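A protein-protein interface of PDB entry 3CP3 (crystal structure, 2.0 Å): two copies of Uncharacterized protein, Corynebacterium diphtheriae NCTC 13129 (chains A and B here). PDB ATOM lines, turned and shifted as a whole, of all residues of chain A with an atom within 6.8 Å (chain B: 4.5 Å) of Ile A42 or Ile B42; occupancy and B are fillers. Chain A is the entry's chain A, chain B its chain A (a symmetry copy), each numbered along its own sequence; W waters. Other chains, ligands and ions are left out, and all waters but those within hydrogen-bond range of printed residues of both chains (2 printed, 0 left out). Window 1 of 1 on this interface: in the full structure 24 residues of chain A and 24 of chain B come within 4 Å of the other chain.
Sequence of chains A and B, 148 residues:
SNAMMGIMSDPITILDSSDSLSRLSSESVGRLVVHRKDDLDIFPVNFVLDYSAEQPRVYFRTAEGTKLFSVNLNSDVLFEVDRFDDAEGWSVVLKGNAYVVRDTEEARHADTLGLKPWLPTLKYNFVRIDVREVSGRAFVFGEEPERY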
ATOM      1  N   ARG A  31      31.210  14.682 -15.271  1.00  0.00           N
ATOM      2  CA  ARG A  31      31.088  13.255 -15.534  1.00  0.00           C
ATOM      3  C   ARG A  31      29.783  12.956 -16.199  1.00  0.00           C
ATOM      4  O   ARG A  31      28.719  13.378 -15.731  1.00  0.00           O
ATOM      5  CB  ARG A  31      31.119  12.506 -14.191  1.00  0.00           C
ATOM      6  CG  ARG A  31      32.475  12.760 -13.503  1.00  0.00           C
ATOM      7  CD  ARG A  31      32.492  12.549 -12.066  1.00  0.00           C
ATOM      8  NE  ARG A  31      33.782  13.068 -11.643  1.00  0.00           N
ATOM      9  CZ  ARG A  31      33.923  14.282 -11.148  1.00  0.00           C
ATOM     10  NH1 ARG A  31      32.825  15.043 -10.896  1.00  0.00           N
ATOM     11  NH2 ARG A  31      35.141  14.688 -10.831  1.00  0.00           N
ATOM     12  N   LEU A  32      29.845  12.197 -17.292  1.00  0.00           N
ATOM     13  CA  LEU A  32      28.642  11.813 -17.953  1.00  0.00           C
ATOM     14  C   LEU A  32      28.258  10.405 -17.508  1.00  0.00           C
ATOM     15  O   LEU A  32      29.073   9.476 -17.581  1.00  0.00           O
ATOM     16  CB  LEU A  32      28.867  11.841 -19.469  1.00  0.00           C
ATOM     17  CG  LEU A  32      27.587  11.673 -20.279  1.00  0.00           C
ATOM     18  CD1 LEU A  32      26.705  12.926 -20.326  1.00  0.00           C
ATOM     19  CD2 LEU A  32      27.970  11.257 -21.686  1.00  0.00           C
ATOM     20  N   VAL A  33      26.985  10.217 -17.118  1.00  0.00           N
ATOM     21  CA  VAL A  33      26.582   8.888 -16.810  1.00  0.00           C
ATOM     22  C   VAL A  33      25.675   8.411 -17.915  1.00  0.00           C
ATOM     23  O   VAL A  33      24.629   9.038 -18.187  1.00  0.00           O
ATOM     24  CB  VAL A  33      25.827   8.814 -15.454  1.00  0.00           C
ATOM     25  CG1 VAL A  33      25.430   7.397 -15.177  1.00  0.00           C
ATOM     26  CG2 VAL A  33      26.740   9.368 -14.326  1.00  0.00           C
ATOM     27  N   VAL A  34      26.042   7.272 -18.485  1.00  0.00           N
ATOM     28  CA  VAL A  34      25.317   6.726 -19.609  1.00  0.00           C
ATOM     29  C   VAL A  34      24.858   5.332 -19.316  1.00  0.00           C
ATOM     30  O   VAL A  34      25.316   4.685 -18.355  1.00  0.00           O
ATOM     31  CB  VAL A  34      26.188   6.659 -20.888  1.00  0.00           C
ATOM     32  CG1 VAL A  34      26.691   8.051 -21.258  1.00  0.00           C
ATOM     33  CG2 VAL A  34      27.378   5.718 -20.668  1.00  0.00           C
ATOM     34  N   LEU A  40      25.557   0.367 -16.977  1.00  0.00           N
ATOM     35  CA  LEU A  40      25.869   1.791 -16.796  1.00  0.00           C
ATOM     36  C   LEU A  40      27.348   2.028 -17.019  1.00  0.00           C
ATOM     37  O   LEU A  40      28.164   1.121 -16.778  1.00  0.00           O
ATOM     38  CB  LEU A  40      25.520   2.246 -15.360  1.00  0.00           C
ATOM     39  CG  LEU A  40      24.055   2.095 -14.877  1.00  0.00           C
ATOM     40  CD1 LEU A  40      23.872   2.655 -13.442  1.00  0.00           C
ATOM     41  CD2 LEU A  40      23.066   2.780 -15.807  1.00  0.00           C
ATOM     42  N   ASP A  41      27.707   3.244 -17.410  1.00  0.00           N
ATOM     43  CA  ASP A  41      29.109   3.660 -17.386  1.00  0.00           C
ATOM     44  C   ASP A  41      29.150   5.114 -17.094  1.00  0.00           C
ATOM     45  O   ASP A  41      28.117   5.794 -17.098  1.00  0.00           O
ATOM     46  CB  ASP A  41      29.844   3.303 -18.701  1.00  0.00           C
ATOM     47  CG  ASP A  41      31.397   3.383 -18.566  1.00  0.00           C
ATOM     48  OD1 ASP A  41      31.964   3.344 -17.439  1.00  0.00           O
ATOM     49  OD2 ASP A  41      32.049   3.536 -19.614  1.00  0.00           O
ATOM     50  N   ILE A  42      30.336   5.585 -16.779  1.00  0.00           N
ATOM     51  CA  ILE A  42      30.525   6.936 -16.427  1.00  0.00           C
ATOM     52  C   ILE A  42      31.947   7.353 -16.825  1.00  0.00           C
ATOM     53  O   ILE A  42      32.912   6.577 -16.676  1.00  0.00           O
ATOM     54  CB  ILE A  42      30.320   7.134 -14.907  1.00  0.00           C
ATOM     55  CG1 ILE A  42      30.607   8.565 -14.501  1.00  0.00           C
ATOM     56  CG2 ILE A  42      31.121   6.116 -14.096  1.00  0.00           C
ATOM     57  CD1 ILE A  42      30.344   8.732 -12.958  1.00  0.00           C
ATOM     58  N   PHE A  43      32.056   8.566 -17.366  1.00  0.00           N
ATOM     59  CA  PHE A  43      33.361   9.046 -17.744  1.00  0.00           C
ATOM     60  C   PHE A  43      33.447  10.558 -17.676  1.00  0.00           C
ATOM     61  O   PHE A  43      32.479  11.244 -17.936  1.00  0.00           O
ATOM     62  CB  PHE A  43      33.753   8.517 -19.125  1.00  0.00           C
ATOM     63  CG  PHE A  43      32.747   8.752 -20.150  1.00  0.00           C
ATOM     64  CD1 PHE A  43      32.754   9.933 -20.881  1.00  0.00           C
ATOM     65  CD2 PHE A  43      31.771   7.789 -20.395  1.00  0.00           C
ATOM     66  CE1 PHE A  43      31.786  10.138 -21.853  1.00  0.00           C
ATOM     67  CE2 PHE A  43      30.825   7.975 -21.302  1.00  0.00           C
ATOM     68  CZ  PHE A  43      30.813   9.137 -22.055  1.00  0.00           C
ATOM     69  N   PRO A  44      34.623  11.070 -17.339  1.00  0.00           N
ATOM     70  CA  PRO A  44      34.820  12.518 -17.190  1.00  0.00           C
ATOM     71  C   PRO A  44      35.011  13.152 -18.562  1.00  0.00           C
ATOM     72  O   PRO A  44      35.536  12.487 -19.478  1.00  0.00           O
ATOM     73  CB  PRO A  44      36.096  12.614 -16.362  1.00  0.00           C
ATOM     74  CG  PRO A  44      36.760  11.338 -16.514  1.00  0.00           C
ATOM     75  CD  PRO A  44      35.844  10.311 -17.046  1.00  0.00           C
ATOM     76  N   LEU A  68      33.096   6.060 -26.361  1.00  0.00           N
ATOM     77  CA  LEU A  68      32.576   6.351 -25.032  1.00  0.00           C
ATOM     78  C   LEU A  68      31.102   6.766 -25.054  1.00  0.00           C
ATOM     79  O   LEU A  68      30.309   6.187 -24.298  1.00  0.00           O
ATOM     80  CB  LEU A  68      33.399   7.440 -24.354  1.00  0.00           C
ATOM     81  CG  LEU A  68      34.850   7.127 -23.982  1.00  0.00           C
ATOM     82  CD1 LEU A  68      35.635   8.434 -23.869  1.00  0.00           C
ATOM     83  CD2 LEU A  68      34.898   6.331 -22.689  1.00  0.00           C
ATOM     84  N   LEU A  78      22.901  11.444 -17.194  1.00  0.00           N
ATOM     85  CA  LEU A  78      23.096  12.420 -16.157  1.00  0.00           C
ATOM     86  C   LEU A  78      24.420  13.060 -16.403  1.00  0.00           C
ATOM     87  O   LEU A  78      25.307  12.436 -16.992  1.00  0.00           O
ATOM     88  CB  LEU A  78      23.245  11.735 -14.771  1.00  0.00           C
ATOM     89  CG  LEU A  78      22.212  10.795 -14.263  1.00  0.00           C
ATOM     90  CD1 LEU A  78      22.710  10.283 -12.879  1.00  0.00           C
ATOM     91  CD2 LEU A  78      20.824  11.502 -14.181  1.00  0.00           C
ATOM     92  N   PHE A  79      24.575  14.276 -15.925  1.00  0.00           N
ATOM     93  CA  PHE A  79      25.852  14.973 -15.958  1.00  0.00           C
ATOM     94  C   PHE A  79      26.105  15.557 -14.586  1.00  0.00           C
ATOM     95  O   PHE A  79      25.228  16.261 -14.007  1.00  0.00           O
ATOM     96  CB  PHE A  79      25.864  16.059 -17.063  1.00  0.00           C
ATOM     97  CG  PHE A  79      27.245  16.619 -17.338  1.00  0.00           C
ATOM     98  CD1 PHE A  79      28.148  15.908 -18.109  1.00  0.00           C
ATOM     99  CD2 PHE A  79      27.662  17.823 -16.783  1.00  0.00           C
ATOM    100  CE1 PHE A  79      29.438  16.413 -18.338  1.00  0.00           C
ATOM    101  CE2 PHE A  79      28.943  18.310 -17.002  1.00  0.00           C
ATOM    102  CZ  PHE A  79      29.818  17.597 -17.773  1.00  0.00           C
ATOM    103  N   GLU A  80      27.291  15.294 -14.044  1.00  0.00           N
ATOM    104  CA  GLU A  80      27.585  15.621 -12.690  1.00  0.00           C
ATOM    105  C   GLU A  80      28.910  16.359 -12.549  1.00  0.00           C
ATOM    106  O   GLU A  80      29.923  16.029 -13.190  1.00  0.00           O
ATOM    107  CB  GLU A  80      27.571  14.343 -11.773  1.00  0.00           C
ATOM    108  CG  GLU A  80      27.624  14.645 -10.258  1.00  0.00           C
ATOM    109  CD  GLU A  80      29.025  14.559  -9.669  1.00  0.00           C
ATOM    110  OE1 GLU A  80      30.012  14.334 -10.461  1.00  0.00           O
ATOM    111  OE2 GLU A  80      29.117  14.550  -8.416  1.00  0.00           O
ATOM    112  N   ASP A  82      31.198  17.927  -9.022  1.00  0.00           N
ATOM    113  CA  ASP A  82      31.265  18.059  -7.572  1.00  0.00           C
ATOM    114  C   ASP A  82      32.559  18.715  -7.071  1.00  0.00           C
ATOM    115  O   ASP A  82      33.423  19.054  -7.905  1.00  0.00           O
ATOM    116  CB  ASP A  82      30.911  16.777  -6.715  1.00  0.00           C
ATOM    117  CG  ASP A  82      31.876  15.535  -6.941  1.00  0.00           C
ATOM    118  OD1 ASP A  82      32.933  15.366  -6.252  1.00  0.00           O
ATOM    119  OD2 ASP A  82      31.465  14.649  -7.679  1.00  0.00           O
ATOM    120  N   SER A  91      27.599  18.986  -4.841  1.00  0.00           N
ATOM    121  CA  SER A  91      27.523  18.366  -6.157  1.00  0.00           C
ATOM    122  C   SER A  91      26.338  18.929  -6.883  1.00  0.00           C
ATOM    123  O   SER A  91      25.366  19.316  -6.243  1.00  0.00           O
ATOM    124  CB  SER A  91      27.289  16.844  -6.053  1.00  0.00           C
ATOM    125  OG  SER A  91      26.087  16.599  -5.334  1.00  0.00           O
ATOM    126  N   VAL A  92      26.399  18.934  -8.205  1.00  0.00           N
ATOM    127  CA  VAL A  92      25.288  19.362  -9.028  1.00  0.00           C
ATOM    128  C   VAL A  92      25.102  18.203 -10.033  1.00  0.00           C
ATOM    129  O   VAL A  92      26.108  17.752 -10.623  1.00  0.00           O
ATOM    130  CB  VAL A  92      25.599  20.665  -9.762  1.00  0.00           C
ATOM    131  CG1 VAL A  92      24.454  21.009 -10.839  1.00  0.00           C
ATOM    132  CG2 VAL A  92      25.720  21.838  -8.695  1.00  0.00           C
ATOM    133  N   VAL A  93      23.862  17.736 -10.158  1.00  0.00           N
ATOM    134  CA  VAL A  93      23.488  16.668 -11.116  1.00  0.00           C
ATOM    135  C   VAL A  93      22.489  17.258 -12.100  1.00  0.00           C
ATOM    136  O   VAL A  93      21.385  17.779 -11.709  1.00  0.00           O
ATOM    137  CB  VAL A  93      22.882  15.476 -10.380  1.00  0.00           C
ATOM    138  CG1 VAL A  93      22.318  14.335 -11.391  1.00  0.00           C
ATOM    139  CG2 VAL A  93      23.858  14.906  -9.423  1.00  0.00           C
ATOM    140  N   ARG A 137      23.297  20.013  -4.384  1.00  0.00           N
ATOM    141  CA  ARG A 137      23.243  19.677  -2.963  1.00  0.00           C
ATOM    142  C   ARG A 137      24.543  20.106  -2.336  1.00  0.00           C
ATOM    143  O   ARG A 137      25.583  20.005  -2.975  1.00  0.00           O
ATOM    144  CB  ARG A 137      23.112  18.149  -2.833  1.00  0.00           C
ATOM    145  CG  ARG A 137      21.824  17.618  -3.402  1.00  0.00           C
ATOM    146  CD  ARG A 137      21.712  16.114  -3.235  1.00  0.00           C
ATOM    147  NE  ARG A 137      22.259  15.404  -4.378  1.00  0.00           N
ATOM    148  CZ  ARG A 137      21.828  14.197  -4.771  1.00  0.00           C
ATOM    149  NH1 ARG A 137      20.851  13.591  -4.109  1.00  0.00           N
ATOM    150  NH2 ARG A 137      22.369  13.607  -5.834  1.00  0.00           N
ATOM    151  N   PHE A 139      26.589  19.183   1.249  1.00  0.00           N
ATOM    152  CA  PHE A 139      26.678  18.236   2.342  1.00  0.00           C
ATOM    153  C   PHE A 139      27.605  18.779   3.429  1.00  0.00           C
ATOM    154  O   PHE A 139      28.742  19.082   3.128  1.00  0.00           O
ATOM    155  CB  PHE A 139      27.298  16.949   1.772  1.00  0.00           C
ATOM    156  CG  PHE A 139      26.706  16.494   0.454  1.00  0.00           C
ATOM    157  CD1 PHE A 139      25.752  15.459   0.422  1.00  0.00           C
ATOM    158  CD2 PHE A 139      27.149  17.039  -0.766  1.00  0.00           C
ATOM    159  CE1 PHE A 139      25.221  15.010  -0.808  1.00  0.00           C
ATOM    160  CE2 PHE A 139      26.621  16.621  -1.995  1.00  0.00           C
ATOM    161  CZ  PHE A 139      25.642  15.575  -2.014  1.00  0.00           C
ATOM    162  N   ARG B  31      32.272   8.576  -6.151  1.00  0.00           N
ATOM    163  CA  ARG B  31      30.879   8.814  -6.509  1.00  0.00           C
ATOM    164  C   ARG B  31      30.155   7.517  -6.675  1.00  0.00           C
ATOM    165  O   ARG B  31      30.613   6.619  -7.391  1.00  0.00           O
ATOM    166  CB  ARG B  31      30.841   9.556  -7.854  1.00  0.00           C
ATOM    167  CG  ARG B  31      31.543  10.920  -7.699  1.00  0.00           C
ATOM    168  CD  ARG B  31      32.018  11.518  -8.934  1.00  0.00           C
ATOM    169  NE  ARG B  31      32.825  12.646  -8.499  1.00  0.00           N
ATOM    170  CZ  ARG B  31      34.137  12.575  -8.398  1.00  0.00           C
ATOM    171  NH1 ARG B  31      34.791  11.464  -8.832  1.00  0.00           N
ATOM    172  NH2 ARG B  31      34.786  13.636  -7.949  1.00  0.00           N
ATOM    173  N   LEU B  32      28.992   7.411  -6.033  1.00  0.00           N
ATOM    174  CA  LEU B  32      28.206   6.232  -6.187  1.00  0.00           C
ATOM    175  C   LEU B  32      27.125   6.489  -7.232  1.00  0.00           C
ATOM    176  O   LEU B  32      26.371   7.466  -7.134  1.00  0.00           O
ATOM    177  CB  LEU B  32      27.562   5.875  -4.843  1.00  0.00           C
ATOM    178  CG  LEU B  32      26.888   4.508  -4.833  1.00  0.00           C
ATOM    179  CD1 LEU B  32      27.864   3.328  -4.748  1.00  0.00           C
ATOM    180  CD2 LEU B  32      25.923   4.465  -3.666  1.00  0.00           C
ATOM    181  N   VAL B  33      26.985   5.567  -8.201  1.00  0.00           N
ATOM    182  CA  VAL B  33      25.909   5.733  -9.115  1.00  0.00           C
ATOM    183  C   VAL B  33      24.872   4.683  -8.807  1.00  0.00           C
ATOM    184  O   VAL B  33      25.174   3.470  -8.840  1.00  0.00           O
ATOM    185  CB  VAL B  33      26.375   5.580 -10.589  1.00  0.00           C
ATOM    186  CG1 VAL B  33      25.207   5.767 -11.509  1.00  0.00           C
ATOM    187  CG2 VAL B  33      27.491   6.620 -10.887  1.00  0.00           C
ATOM    188  N   ASP B  41      20.800   8.246 -10.148  1.00  0.00           N
ATOM    189  CA  ASP B  41      21.345   9.361  -9.374  1.00  0.00           C
ATOM    190  C   ASP B  41      22.764   9.055  -9.068  1.00  0.00           C
ATOM    191  O   ASP B  41      23.237   7.933  -9.293  1.00  0.00           O
ATOM    192  CB  ASP B  41      20.516   9.643  -8.098  1.00  0.00           C
ATOM    193  CG  ASP B  41      20.835  11.035  -7.466  1.00  0.00           C
ATOM    194  OD1 ASP B  41      21.386  11.952  -8.134  1.00  0.00           O
ATOM    195  OD2 ASP B  41      20.567  11.183  -6.260  1.00  0.00           O
ATOM    196  N   ILE B  42      23.467  10.066  -8.609  1.00  0.00           N
ATOM    197  CA  ILE B  42      24.840   9.944  -8.321  1.00  0.00           C
ATOM    198  C   ILE B  42      25.195  10.923  -7.195  1.00  0.00           C
ATOM    199  O   ILE B  42      24.696  12.066  -7.153  1.00  0.00           O
ATOM    200  CB  ILE B  42      25.687  10.250  -9.578  1.00  0.00           C
ATOM    201  CG1 ILE B  42      27.167  10.209  -9.260  1.00  0.00           C
ATOM    202  CG2 ILE B  42      25.260  11.562 -10.235  1.00  0.00           C
ATOM    203  CD1 ILE B  42      27.991  10.482 -10.573  1.00  0.00           C
ATOM    204  N   PHE B  43      26.028  10.450  -6.268  1.00  0.00           N
ATOM    205  CA  PHE B  43      26.433  11.314  -5.189  1.00  0.00           C
ATOM    206  C   PHE B  43      27.806  10.949  -4.659  1.00  0.00           C
ATOM    207  O   PHE B  43      28.174   9.791  -4.645  1.00  0.00           O
ATOM    208  CB  PHE B  43      25.381  11.324  -4.078  1.00  0.00           C
ATOM    209  CG  PHE B  43      24.997   9.996  -3.623  1.00  0.00           C
ATOM    210  CD1 PHE B  43      25.702   9.375  -2.600  1.00  0.00           C
ATOM    211  CD2 PHE B  43      23.919   9.346  -4.220  1.00  0.00           C
ATOM    212  CE1 PHE B  43      25.319   8.109  -2.181  1.00  0.00           C
ATOM    213  CE2 PHE B  43      23.553   8.129  -3.850  1.00  0.00           C
ATOM    214  CZ  PHE B  43      24.228   7.489  -2.825  1.00  0.00           C
ATOM    215  N   LEU B  78      27.540   1.566  -9.572  1.00  0.00           N
ATOM    216  CA  LEU B  78      28.899   1.810  -9.972  1.00  0.00           C
ATOM    217  C   LEU B  78      29.509   2.690  -8.934  1.00  0.00           C
ATOM    218  O   LEU B  78      28.795   3.451  -8.273  1.00  0.00           O
ATOM    219  CB  LEU B  78      28.950   2.653 -11.276  1.00  0.00           C
ATOM    220  CG  LEU B  78      28.231   2.218 -12.502  1.00  0.00           C
ATOM    221  CD1 LEU B  78      28.476   3.312 -13.581  1.00  0.00           C
ATOM    222  CD2 LEU B  78      28.725   0.807 -12.950  1.00  0.00           C
ATOM    223  N   GLU B  80      32.902   5.381  -8.725  1.00  0.00           N
ATOM    224  CA  GLU B  80      33.847   6.026  -9.572  1.00  0.00           C
ATOM    225  C   GLU B  80      34.721   7.017  -8.812  1.00  0.00           C
ATOM    226  O   GLU B  80      34.258   7.779  -7.945  1.00  0.00           O
ATOM    227  CB  GLU B  80      33.142   6.739 -10.784  1.00  0.00           C
ATOM    228  CG  GLU B  80      34.109   7.239 -11.880  1.00  0.00           C
ATOM    229  CD  GLU B  80      34.472   8.711 -11.746  1.00  0.00           C
ATOM    230  OE1 GLU B  80      34.029   9.363 -10.732  1.00  0.00           O
ATOM    231  OE2 GLU B  80      35.050   9.247 -12.724  1.00  0.00           O
ATOM    232  N   VAL B  93      36.424   3.011 -12.573  1.00  0.00           N
ATOM    233  CA  VAL B  93      34.999   2.665 -12.352  1.00  0.00           C
ATOM    234  C   VAL B  93      34.946   1.249 -11.799  1.00  0.00           C
ATOM    235  O   VAL B  93      35.452   0.258 -12.436  1.00  0.00           O
ATOM    236  CB  VAL B  93      34.214   2.765 -13.658  1.00  0.00           C
ATOM    237  CG1 VAL B  93      32.678   2.256 -13.508  1.00  0.00           C
ATOM    238  CG2 VAL B  93      34.270   4.145 -14.192  1.00  0.00           C
ATOM    239  N   ARG B 137      41.011   3.894 -16.699  1.00  0.00           N
ATOM    240  CA  ARG B 137      41.361   4.463 -17.999  1.00  0.00           C
ATOM    241  C   ARG B 137      42.182   5.701 -17.757  1.00  0.00           C
ATOM    242  O   ARG B 137      41.925   6.417 -16.797  1.00  0.00           O
ATOM    243  CB  ARG B 137      40.060   4.866 -18.716  1.00  0.00           C
ATOM    244  CG  ARG B 137      39.176   3.691 -19.036  1.00  0.00           C
ATOM    245  CD  ARG B 137      37.916   4.115 -19.766  1.00  0.00           C
ATOM    246  NE  ARG B 137      36.832   4.403 -18.843  1.00  0.00           N
ATOM    247  CZ  ARG B 137      35.537   4.254 -19.157  1.00  0.00           C
ATOM    248  NH1 ARG B 137      35.190   3.820 -20.362  1.00  0.00           N
ATOM    249  NH2 ARG B 137      34.595   4.529 -18.259  1.00  0.00           N
HETATM  250  O   HOH W   1      24.645  14.503  -5.877  1.00  0.00           O
HETATM  251  O   HOH W   2      35.637   6.240 -16.856  1.00  0.00           O
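OD2 of Asp A82 lies within salt-bridge range of NE of Arg B31 (2.6 Å).
OE1 of Glu B80 lies within salt-bridge range of NE of Arg A31.
The guanidinium group of Arg B31 lies close to the guanidinium group of Arg A31.
The guanidinium group (NH2) of Arg A137 is in hydrogen-bond range of the backbone carbonyl oxygen (O) of Ile B42 (3.1 Å).
The side-chain carboxylate (OD1) of Asp A41 lies within salt-bridge range of the guanidinium group (NH2) of Arg B137.
NH2 of Arg B137 sits at hydrogen-bond distance from O of Ile A42.
OD1 of Asp B41 lies within salt-bridge range of NH2 of Arg A137 (3.0 Å).
The guanidinium group of Arg B31 lies within salt-bridge range of the side-chain carboxylate of Glu A80 (3.8 Å).
The guanidinium group (NH1) of Arg A31 is in salt-bridge range of the side-chain carboxylate (OE1) of Glu A80 (2.9 Å).
The side-chain carboxylate (OD2) of Asp A82 lies close to the side-chain carboxylate (OE2) of Glu A80.
O of Ser A91 is in hydrogen-bond range of N of Arg A137 (2.9 Å).
The guanidinium group (NH1) of Arg B31 is in salt-bridge range of the side-chain carboxylate (OE1) of Glu B80 (2.9 Å).
The backbone NH of Val A33 sits at hydrogen-bond distance from the backbone carbonyl oxygen of Leu A78 (2.8 Å).
N of Val B33 sits at hydrogen-bond distance from O of Leu B78.
Among the printed residues, pairs that only touch across the chains: Leu A40 with Val B33 (3.9 Å), Leu A40 with Leu B78 (3.6 Å), Asp A41 with Leu B78 (3.9 Å), Ile A42 with Ile B42 (3.8 Å), Ile A42 with Leu B78 (3.9 Å), Ile A42 with Glu B80 (3.9 Å), Ile A42 with Val B93 (3.7 Å), Leu A68 with Arg B137 (3.4 Å), Leu A78 with Asp B41 (3.9 Å), Leu A78 with Ile B42 (3.9 Å), Glu A80 with Ile B42 (3.9 Å) and Val A93 with Ile B42 (3.7 Å).
Val A33 touches none of the printed residues of chain B.
Printed residues of chain B within 4 Å of Leu A40: Val B33 and Leu B78.
Ile A42 touches just these residues of chain B: Ile B42, Leu B78, Glu B80, Val B93 and Arg B137.
Printed residues of chain B within 4 Å of Glu A80: Arg B31 (3.8 Å) and Ile B42 (3.9 Å).
Printed residues of chain B within 4 Å of Val A93: Ile B42 (3.7 Å).
Phe A139 touches none of the printed residues of chain B.
Of the printed residues of chain A, Arg B31 touches Arg A31, Glu A80 and Asp A82.
Of chain A, only Ile A42 (3.8 Å), Leu A78 (3.9 Å), Glu A80 (3.9 Å), Val A93 (3.7 Å) and Arg A137 (3.1 Å) come within 4 Å of Ile B42.
Printed residues of chain A within 4 Å of Arg B137: Asp A41, Ile A42 and Leu A68.
The nearest residue of chain B that does not touch Ile A42 is Val B33 (4.1 Å).
The nearest printed residue of chain B that does not touch Leu A78 is Val B33 (5.3 Å).
Along chain B the printed residues that touch a printed residue of chain A span positions 31 to 137.
Of the 19 printed residues of chain A, 10 touch a printed residue of chain B.
Printed residues of chain A that touch a printed residue of chain B: Arg A31, Leu A40, Asp A41, Ile A42, Leu A68, Leu A78, Glu A80, Asp A82, Val A93 and Arg A137.
Among the printed residues, Asp or Glu carboxylates within 4 Å of a Lys or Arg side-chain nitrogen of the other chain: Arg A31 with Glu B80 (3.8 Å), Asp A41 with Arg B137 (3.0 Å), Glu A80 with Arg B31 (3.8 Å), Asp A82 with Arg B31 (2.6 Å) and Arg A137 with Asp B41 (3.0 Å).
Arg A31 touches Glu B80, and with the chains exchanged Glu A80 touches Arg B31.
Ile A42 touches its own counterpart, Ile B42.
Ile A42 touches Leu B78, and with the chains exchanged Leu A78 touches Ile B42.
Ile A42 touches Val B93, and with the chains exchanged Val A93 touches Ile B42.
Of the 20 pairs that touch across the chains among the printed residues, 16 have their exchanged pair printed and touching as well.
Water W1 lies within hydrogen-bond range of NH2 of Arg A137 (2.4 Å), OG of Ser A91 (2.6 Å) and O of Ile B42 (2.8 Å).
Water W2 bridges the guanidinium group (NH2) of Arg B137 (2.4 Å) and the backbone carbonyl oxygen (O) of Ile A42 (2.8 Å).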
